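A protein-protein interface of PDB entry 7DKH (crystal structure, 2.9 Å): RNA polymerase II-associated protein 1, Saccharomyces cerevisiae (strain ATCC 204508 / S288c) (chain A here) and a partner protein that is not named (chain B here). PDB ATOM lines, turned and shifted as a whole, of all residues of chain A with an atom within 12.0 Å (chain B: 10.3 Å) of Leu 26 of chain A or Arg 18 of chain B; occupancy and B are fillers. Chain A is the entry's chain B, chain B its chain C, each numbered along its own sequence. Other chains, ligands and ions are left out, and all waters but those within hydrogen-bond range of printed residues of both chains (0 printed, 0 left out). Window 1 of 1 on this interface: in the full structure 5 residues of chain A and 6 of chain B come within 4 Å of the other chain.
The backbone NH (N) of Arg 18 of chain B is in hydrogen-bond range of the backbone carbonyl oxygen (O) of Leu 26 of chain A (2.8 Å).
The backbone NH (N) of Val 28 of chain A is in hydrogen-bond range of the backbone carbonyl oxygen (O) of His 16 of chain B, 3.1 Å away.
OE1 of Glu 17 of chain B lies within salt-bridge range of NZ of Lys 25 of chain A (3.1 Å).
The backbone carbonyl oxygen of Glu 12 of chain B lies within hydrogen-bond range of a ring nitrogen (ND1) of His 16 of chain B, at 2.9 Å.
Among the printed residues, pairs that only touch across the chains: Leu 27 of chain A with His 16 of chain B (3.2 Å), Leu 26 of chain A with Glu 17 of chain B (3.3 Å), Pro 23 of chain A with Val 21 of chain B (3.4 Å), Leu 26 of chain A with Leu 20 of chain B (3.7 Å), Val 28 of chain A with Glu 17 of chain B (3.9 Å), Lys 25 of chain A with Ile 19 of chain B (3.9 Å), Leu 26 of chain A with His 16 of chain B (3.9 Å) and Lys 25 of chain A with Arg 18 of chain B (3.99 Å).
Of the printed residues of chain A, Arg 18 of chain B touches Lys 25 and Leu 26.
Leu 27 of chain A touches just one residue of chain B: His 16 (3.2 Å).
Glu 17 of chain B touches just these residues of chain A: Lys 25, Leu 26 and Val 28.
Of chain A, only Lys 25 comes within 4 Å of Ile 19 of chain B.
Leu 20 of chain B touches just one residue of chain A: Leu 26.
Printed residues of chain A within 4 Å of His 16 of chain B: Leu 26 (3.9 Å), Leu 27 (3.2 Å) and Val 28 (3.1 Å).
Of the printed residues of chain B, Pro 23 of chain A touches Val 21 (3.4 Å).
Printed residues of chain A within 4 Å of Val 21 of chain B: Pro 23 (3.4 Å).
Ser 25 of chain B touches none of the printed residues of chain A.
Tyr 29 of chain A touches none of the printed residues of chain B.
The nearest residue of chain B that does not touch Leu 26 of chain A is Ile 19 of chain B (4.4 Å).
The nearest printed residue of chain A that does not touch Arg 18 of chain B is Val 28 of chain A (4.3 Å).
Of the 12 printed residues of chain B, 6 touch a printed residue of chain A.
Hydrophobic or aromatic side chains of chain B that line the printed part of chain A: Ile 19, Leu 20 and Val 21.
Of the 11 printed residues of chain A, 5 touch a printed residue of chain B.
Hydrophobic or aromatic side chains of chain A that line the printed part of chain B: Pro 23, Leu 26, Leu 27 and Val 28.
Along chain A the printed residues that touch a printed residue of chain B span positions 23 to 28.
Among the printed residues, 11 pairs touch across the chains.
Among the printed residues, Asp or Glu carboxylates within 4 Å of a Lys or Arg side-chain nitrogen of the other chain: Lys 25 of chain A with Glu 17 of chain B (3.1 Å).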
ATOM      1  N   GLN A  21     -10.848   9.242  11.211  1.00  0.00           N
ATOM      2  CA  GLN A  21     -12.116   9.671  11.807  1.00  0.00           C
ATOM      3  C   GLN A  21     -12.290   9.127  13.222  1.00  0.00           C
ATOM      4  O   GLN A  21     -13.179   8.324  13.507  1.00  0.00           O
ATOM      5  CB  GLN A  21     -13.298   9.267  10.924  1.00  0.00           C
ATOM      6  CG  GLN A  21     -13.512  10.169   9.730  1.00  0.00           C
ATOM      7  CD  GLN A  21     -14.952  10.617   9.573  1.00  0.00           C
ATOM      8  OE1 GLN A  21     -15.402  11.566  10.221  1.00  0.00           O
ATOM      9  NE2 GLN A  21     -15.687   9.929   8.704  1.00  0.00           N
ATOM     10  N   LEU A  22     -11.418   9.589  14.099  1.00  0.00           N
ATOM     11  CA  LEU A  22     -11.318   9.130  15.476  1.00  0.00           C
ATOM     12  C   LEU A  22     -12.578   9.517  16.240  1.00  0.00           C
ATOM     13  O   LEU A  22     -12.697  10.677  16.652  1.00  0.00           O
ATOM     14  CB  LEU A  22     -10.085   9.761  16.107  1.00  0.00           C
ATOM     15  CG  LEU A  22      -8.795   9.469  15.331  1.00  0.00           C
ATOM     16  CD1 LEU A  22      -7.855  10.658  15.409  1.00  0.00           C
ATOM     17  CD2 LEU A  22      -8.104   8.205  15.846  1.00  0.00           C
ATOM     18  N   PRO A  23     -13.515   8.603  16.484  1.00  0.00           N
ATOM     19  CA  PRO A  23     -14.776   8.993  17.132  1.00  0.00           C
ATOM     20  C   PRO A  23     -14.562   9.308  18.604  1.00  0.00           C
ATOM     21  O   PRO A  23     -13.452   9.128  19.128  1.00  0.00           O
ATOM     22  CB  PRO A  23     -15.656   7.746  16.943  1.00  0.00           C
ATOM     23  CG  PRO A  23     -14.665   6.608  16.964  1.00  0.00           C
ATOM     24  CD  PRO A  23     -13.412   7.142  16.303  1.00  0.00           C
ATOM     25  N   PRO A  24     -15.594   9.795  19.301  1.00  0.00           N
ATOM     26  CA  PRO A  24     -15.458  10.050  20.740  1.00  0.00           C
ATOM     27  C   PRO A  24     -15.014   8.800  21.485  1.00  0.00           C
ATOM     28  O   PRO A  24     -15.318   7.673  21.087  1.00  0.00           O
ATOM     29  CB  PRO A  24     -16.868  10.485  21.157  1.00  0.00           C
ATOM     30  CG  PRO A  24     -17.433  11.105  19.939  1.00  0.00           C
ATOM     31  CD  PRO A  24     -16.850  10.353  18.769  1.00  0.00           C
ATOM     32  N   LYS A  25     -14.297   9.016  22.584  1.00  0.00           N
ATOM     33  CA  LYS A  25     -13.704   7.933  23.354  1.00  0.00           C
ATOM     34  C   LYS A  25     -14.655   7.437  24.430  1.00  0.00           C
ATOM     35  O   LYS A  25     -15.317   8.230  25.105  1.00  0.00           O
ATOM     36  CB  LYS A  25     -12.408   8.393  24.021  1.00  0.00           C
ATOM     37  CG  LYS A  25     -11.563   9.289  23.153  1.00  0.00           C
ATOM     38  CD  LYS A  25     -10.800   8.477  22.126  1.00  0.00           C
ATOM     39  CE  LYS A  25      -9.727   9.308  21.453  1.00  0.00           C
ATOM     40  NZ  LYS A  25      -8.670   9.748  22.406  1.00  0.00           N
ATOM     41  N   LEU A  26     -14.693   6.119  24.604  1.00  0.00           N
ATOM     42  CA  LEU A  26     -15.376   5.540  25.744  1.00  0.00           C
ATOM     43  C   LEU A  26     -14.482   5.620  26.975  1.00  0.00           C
ATOM     44  O   LEU A  26     -13.261   5.771  26.882  1.00  0.00           O
ATOM     45  CB  LEU A  26     -15.749   4.083  25.476  1.00  0.00           C
ATOM     46  CG  LEU A  26     -16.569   3.769  24.225  1.00  0.00           C
ATOM     47  CD1 LEU A  26     -16.172   2.411  23.664  1.00  0.00           C
ATOM     48  CD2 LEU A  26     -18.054   3.817  24.537  1.00  0.00           C
ATOM     49  N   LEU A  27     -15.107   5.517  28.140  1.00  0.00           N
ATOM     50  CA  LEU A  27     -14.391   5.422  29.400  1.00  0.00           C
ATOM     51  C   LEU A  27     -14.578   4.025  29.972  1.00  0.00           C
ATOM     52  O   LEU A  27     -15.671   3.455  29.891  1.00  0.00           O
ATOM     53  CB  LEU A  27     -14.891   6.475  30.391  1.00  0.00           C
ATOM     54  CG  LEU A  27     -14.708   7.933  29.956  1.00  0.00           C
ATOM     55  CD1 LEU A  27     -15.602   8.874  30.751  1.00  0.00           C
ATOM     56  CD2 LEU A  27     -13.250   8.343  30.090  1.00  0.00           C
ATOM     57  N   VAL A  28     -13.505   3.466  30.538  1.00  0.00           N
ATOM     58  CA  VAL A  28     -13.619   2.181  31.216  1.00  0.00           C
ATOM     59  C   VAL A  28     -14.483   2.378  32.454  1.00  0.00           C
ATOM     60  O   VAL A  28     -14.347   3.374  33.181  1.00  0.00           O
ATOM     61  CB  VAL A  28     -12.234   1.594  31.561  1.00  0.00           C
ATOM     62  CG1 VAL A  28     -11.267   1.761  30.399  1.00  0.00           C
ATOM     63  CG2 VAL A  28     -11.665   2.187  32.837  1.00  0.00           C
ATOM     64  N   TYR A  29     -15.409   1.457  32.677  1.00  0.00           N
ATOM     65  CA  TYR A  29     -16.288   1.581  33.825  1.00  0.00           C
ATOM     66  C   TYR A  29     -15.512   1.382  35.124  1.00  0.00           C
ATOM     67  O   TYR A  29     -14.548   0.615  35.170  1.00  0.00           O
ATOM     68  CB  TYR A  29     -17.423   0.571  33.741  1.00  0.00           C
ATOM     69  CG  TYR A  29     -18.294   0.770  32.527  1.00  0.00           C
ATOM     70  CD1 TYR A  29     -19.172   1.840  32.451  1.00  0.00           C
ATOM     71  CD2 TYR A  29     -18.239  -0.112  31.457  1.00  0.00           C
ATOM     72  CE1 TYR A  29     -19.973   2.030  31.338  1.00  0.00           C
ATOM     73  CE2 TYR A  29     -19.039   0.068  30.340  1.00  0.00           C
ATOM     74  CZ  TYR A  29     -19.906   1.141  30.287  1.00  0.00           C
ATOM     75  OH  TYR A  29     -20.704   1.329  29.178  1.00  0.00           O
ATOM     76  N   PRO A  30     -15.898   2.085  36.188  1.00  0.00           N
ATOM     77  CA  PRO A  30     -15.273   1.837  37.489  1.00  0.00           C
ATOM     78  C   PRO A  30     -15.561   0.418  37.956  1.00  0.00           C
ATOM     79  O   PRO A  30     -16.613  -0.156  37.660  1.00  0.00           O
ATOM     80  CB  PRO A  30     -15.924   2.880  38.409  1.00  0.00           C
ATOM     81  CG  PRO A  30     -17.175   3.291  37.713  1.00  0.00           C
ATOM     82  CD  PRO A  30     -16.896   3.163  36.247  1.00  0.00           C
ATOM     83  N   GLU A  31     -14.603  -0.146  38.688  1.00  0.00           N
ATOM     84  CA  GLU A  31     -14.719  -1.526  39.141  1.00  0.00           C
ATOM     85  C   GLU A  31     -15.914  -1.720  40.065  1.00  0.00           C
ATOM     86  O   GLU A  31     -16.181  -0.903  40.951  1.00  0.00           O
ATOM     87  CB  GLU A  31     -13.440  -1.968  39.851  1.00  0.00           C
ATOM     88  CG  GLU A  31     -12.392  -2.537  38.919  1.00  0.00           C
ATOM     89  CD  GLU A  31     -11.389  -3.416  39.644  1.00  0.00           C
ATOM     90  OE1 GLU A  31     -10.915  -4.400  39.036  1.00  0.00           O
ATOM     91  OE2 GLU A  31     -11.068  -3.127  40.818  1.00  0.00           O
ATOM     92  N   GLU B  12      -2.667   9.377  32.310  1.00  0.00           N
ATOM     93  CA  GLU B  12      -3.810   8.884  33.063  1.00  0.00           C
ATOM     94  C   GLU B  12      -5.129   9.059  32.319  1.00  0.00           C
ATOM     95  O   GLU B  12      -6.137   8.483  32.740  1.00  0.00           O
ATOM     96  CB  GLU B  12      -3.896   9.569  34.428  1.00  0.00           C
ATOM     97  CG  GLU B  12      -4.490   8.659  35.493  1.00  0.00           C
ATOM     98  CD  GLU B  12      -5.179   9.414  36.607  1.00  0.00           C
ATOM     99  OE1 GLU B  12      -5.872  10.410  36.314  1.00  0.00           O
ATOM    100  OE2 GLU B  12      -5.022   9.011  37.780  1.00  0.00           O
ATOM    101  N   THR B  13      -5.157   9.828  31.226  1.00  0.00           N
ATOM    102  CA  THR B  13      -6.353   9.835  30.390  1.00  0.00           C
ATOM    103  C   THR B  13      -6.471   8.556  29.568  1.00  0.00           C
ATOM    104  O   THR B  13      -7.563   7.987  29.461  1.00  0.00           O
ATOM    105  CB  THR B  13      -6.372  11.061  29.475  1.00  0.00           C
ATOM    106  OG1 THR B  13      -5.952  12.217  30.209  1.00  0.00           O
ATOM    107  CG2 THR B  13      -7.773  11.280  28.905  1.00  0.00           C
ATOM    108  N   MET B  14      -5.369   8.085  28.985  1.00  0.00           N
ATOM    109  CA  MET B  14      -5.386   6.830  28.231  1.00  0.00           C
ATOM    110  C   MET B  14      -5.759   5.633  29.107  1.00  0.00           C
ATOM    111  O   MET B  14      -6.429   4.717  28.636  1.00  0.00           O
ATOM    112  CB  MET B  14      -4.038   6.572  27.554  1.00  0.00           C
ATOM    113  CG  MET B  14      -3.259   7.815  27.199  1.00  0.00           C
ATOM    114  SD  MET B  14      -3.974   8.688  25.611  1.00  0.00           S
ATOM    115  CE  MET B  14      -3.088   7.600  24.258  1.00  0.00           C
ATOM    116  N   LYS B  15      -5.320   5.644  30.372  1.00  0.00           N
ATOM    117  CA  LYS B  15      -5.633   4.538  31.276  1.00  0.00           C
ATOM    118  C   LYS B  15      -7.134   4.370  31.451  1.00  0.00           C
ATOM    119  O   LYS B  15      -7.621   3.249  31.650  1.00  0.00           O
ATOM    120  CB  LYS B  15      -5.010   4.784  32.649  1.00  0.00           C
ATOM    121  CG  LYS B  15      -3.544   4.459  32.774  1.00  0.00           C
ATOM    122  CD  LYS B  15      -3.019   5.060  34.066  1.00  0.00           C
ATOM    123  CE  LYS B  15      -1.521   5.285  34.008  1.00  0.00           C
ATOM    124  NZ  LYS B  15      -1.050   6.139  35.136  1.00  0.00           N
ATOM    125  N   HIS B  16      -7.879   5.469  31.376  1.00  0.00           N
ATOM    126  CA  HIS B  16      -9.321   5.456  31.556  1.00  0.00           C
ATOM    127  C   HIS B  16     -10.093   5.530  30.249  1.00  0.00           C
ATOM    128  O   HIS B  16     -11.322   5.639  30.284  1.00  0.00           O
ATOM    129  CB  HIS B  16      -9.737   6.612  32.468  1.00  0.00           C
ATOM    130  CG  HIS B  16      -9.165   6.519  33.845  1.00  0.00           C
ATOM    131  ND1 HIS B  16      -8.338   7.486  34.371  1.00  0.00           N
ATOM    132  CD2 HIS B  16      -9.298   5.574  34.805  1.00  0.00           C
ATOM    133  CE1 HIS B  16      -7.991   7.143  35.598  1.00  0.00           C
ATOM    134  NE2 HIS B  16      -8.559   5.986  35.885  1.00  0.00           N
ATOM    135  N   GLU B  17      -9.418   5.506  29.106  1.00  0.00           N
ATOM    136  CA  GLU B  17     -10.102   5.554  27.823  1.00  0.00           C
ATOM    137  C   GLU B  17     -10.168   4.164  27.197  1.00  0.00           C
ATOM    138  O   GLU B  17      -9.314   3.311  27.444  1.00  0.00           O
ATOM    139  CB  GLU B  17      -9.410   6.534  26.873  1.00  0.00           C
ATOM    140  CG  GLU B  17      -9.704   8.009  27.150  1.00  0.00           C
ATOM    141  CD  GLU B  17      -9.112   8.912  26.081  1.00  0.00           C
ATOM    142  OE1 GLU B  17      -8.367   8.387  25.225  1.00  0.00           O
ATOM    143  OE2 GLU B  17      -9.374  10.135  26.098  1.00  0.00           O
ATOM    144  N   ARG B  18     -11.219   3.933  26.412  1.00  0.00           N
ATOM    145  CA  ARG B  18     -11.366   2.731  25.601  1.00  0.00           C
ATOM    146  C   ARG B  18     -11.790   3.149  24.202  1.00  0.00           C
ATOM    147  O   ARG B  18     -12.682   3.986  24.039  1.00  0.00           O
ATOM    148  CB  ARG B  18     -12.379   1.741  26.196  1.00  0.00           C
ATOM    149  CG  ARG B  18     -12.000   0.271  26.005  1.00  0.00           C
ATOM    150  CD  ARG B  18     -13.075  -0.686  26.511  1.00  0.00           C
ATOM    151  NE  ARG B  18     -14.270  -0.645  25.679  1.00  0.00           N
ATOM    152  CZ  ARG B  18     -15.502  -0.418  26.121  1.00  0.00           C
ATOM    153  NH1 ARG B  18     -15.732  -0.211  27.410  1.00  0.00           N
ATOM    154  NH2 ARG B  18     -16.512  -0.408  25.265  1.00  0.00           N
ATOM    155  N   ILE B  19     -11.156   2.561  23.195  1.00  0.00           N
ATOM    156  CA  ILE B  19     -11.336   2.995  21.816  1.00  0.00           C
ATOM    157  C   ILE B  19     -12.545   2.284  21.224  1.00  0.00           C
ATOM    158  O   ILE B  19     -12.566   1.055  21.111  1.00  0.00           O
ATOM    159  CB  ILE B  19     -10.075   2.718  20.986  1.00  0.00           C
ATOM    160  CG1 ILE B  19      -8.894   3.489  21.570  1.00  0.00           C
ATOM    161  CG2 ILE B  19     -10.292   3.107  19.539  1.00  0.00           C
ATOM    162  CD1 ILE B  19      -9.216   4.947  21.846  1.00  0.00           C
ATOM    163  N   LEU B  20     -13.545   3.073  20.834  1.00  0.00           N
ATOM    164  CA  LEU B  20     -14.763   2.533  20.241  1.00  0.00           C
ATOM    165  C   LEU B  20     -14.498   2.004  18.838  1.00  0.00           C
ATOM    166  O   LEU B  20     -14.818   0.856  18.526  1.00  0.00           O
ATOM    167  CB  LEU B  20     -15.849   3.607  20.211  1.00  0.00           C
ATOM    168  CG  LEU B  20     -17.131   3.242  19.452  1.00  0.00           C
ATOM    169  CD1 LEU B  20     -17.780   1.958  19.976  1.00  0.00           C
ATOM    170  CD2 LEU B  20     -18.095   4.409  19.510  1.00  0.00           C
ATOM    171  N   VAL B  21     -13.893   2.822  17.985  1.00  0.00           N
ATOM    172  CA  VAL B  21     -13.555   2.438  16.620  1.00  0.00           C
ATOM    173  C   VAL B  21     -12.151   2.940  16.334  1.00  0.00           C
ATOM    174  O   VAL B  21     -11.832   4.098  16.628  1.00  0.00           O
ATOM    175  CB  VAL B  21     -14.537   3.047  15.597  1.00  0.00           C
ATOM    176  CG1 VAL B  21     -14.057   2.800  14.180  1.00  0.00           C
ATOM    177  CG2 VAL B  21     -15.943   2.508  15.802  1.00  0.00           C
ATOM    178  N   ASP B  22     -11.308   2.078  15.763  1.00  0.00           N
ATOM    179  CA  ASP B  22      -9.975   2.491  15.351  1.00  0.00           C
ATOM    180  C   ASP B  22      -9.898   2.564  13.824  1.00  0.00           C
ATOM    181  O   ASP B  22     -10.894   2.366  13.120  1.00  0.00           O
ATOM    182  CB  ASP B  22      -8.912   1.561  15.960  1.00  0.00           C
ATOM    183  CG  ASP B  22      -8.980   0.138  15.432  1.00  0.00           C
ATOM    184  OD1 ASP B  22      -9.857  -0.184  14.595  1.00  0.00           O
ATOM    185  OD2 ASP B  22      -8.146  -0.675  15.875  1.00  0.00           O
ATOM    186  N   SER B  25     -10.938  -1.107  12.390  1.00  0.00           N
ATOM    187  CA  SER B  25     -12.319  -1.568  12.521  1.00  0.00           C
ATOM    188  C   SER B  25     -13.293  -0.671  11.774  1.00  0.00           C
ATOM    189  O   SER B  25     -14.383  -1.122  11.407  1.00  0.00           O
ATOM    190  CB  SER B  25     -12.717  -1.664  13.997  1.00  0.00           C
ATOM    191  OG  SER B  25     -12.291  -0.527  14.723  1.00  0.00           O
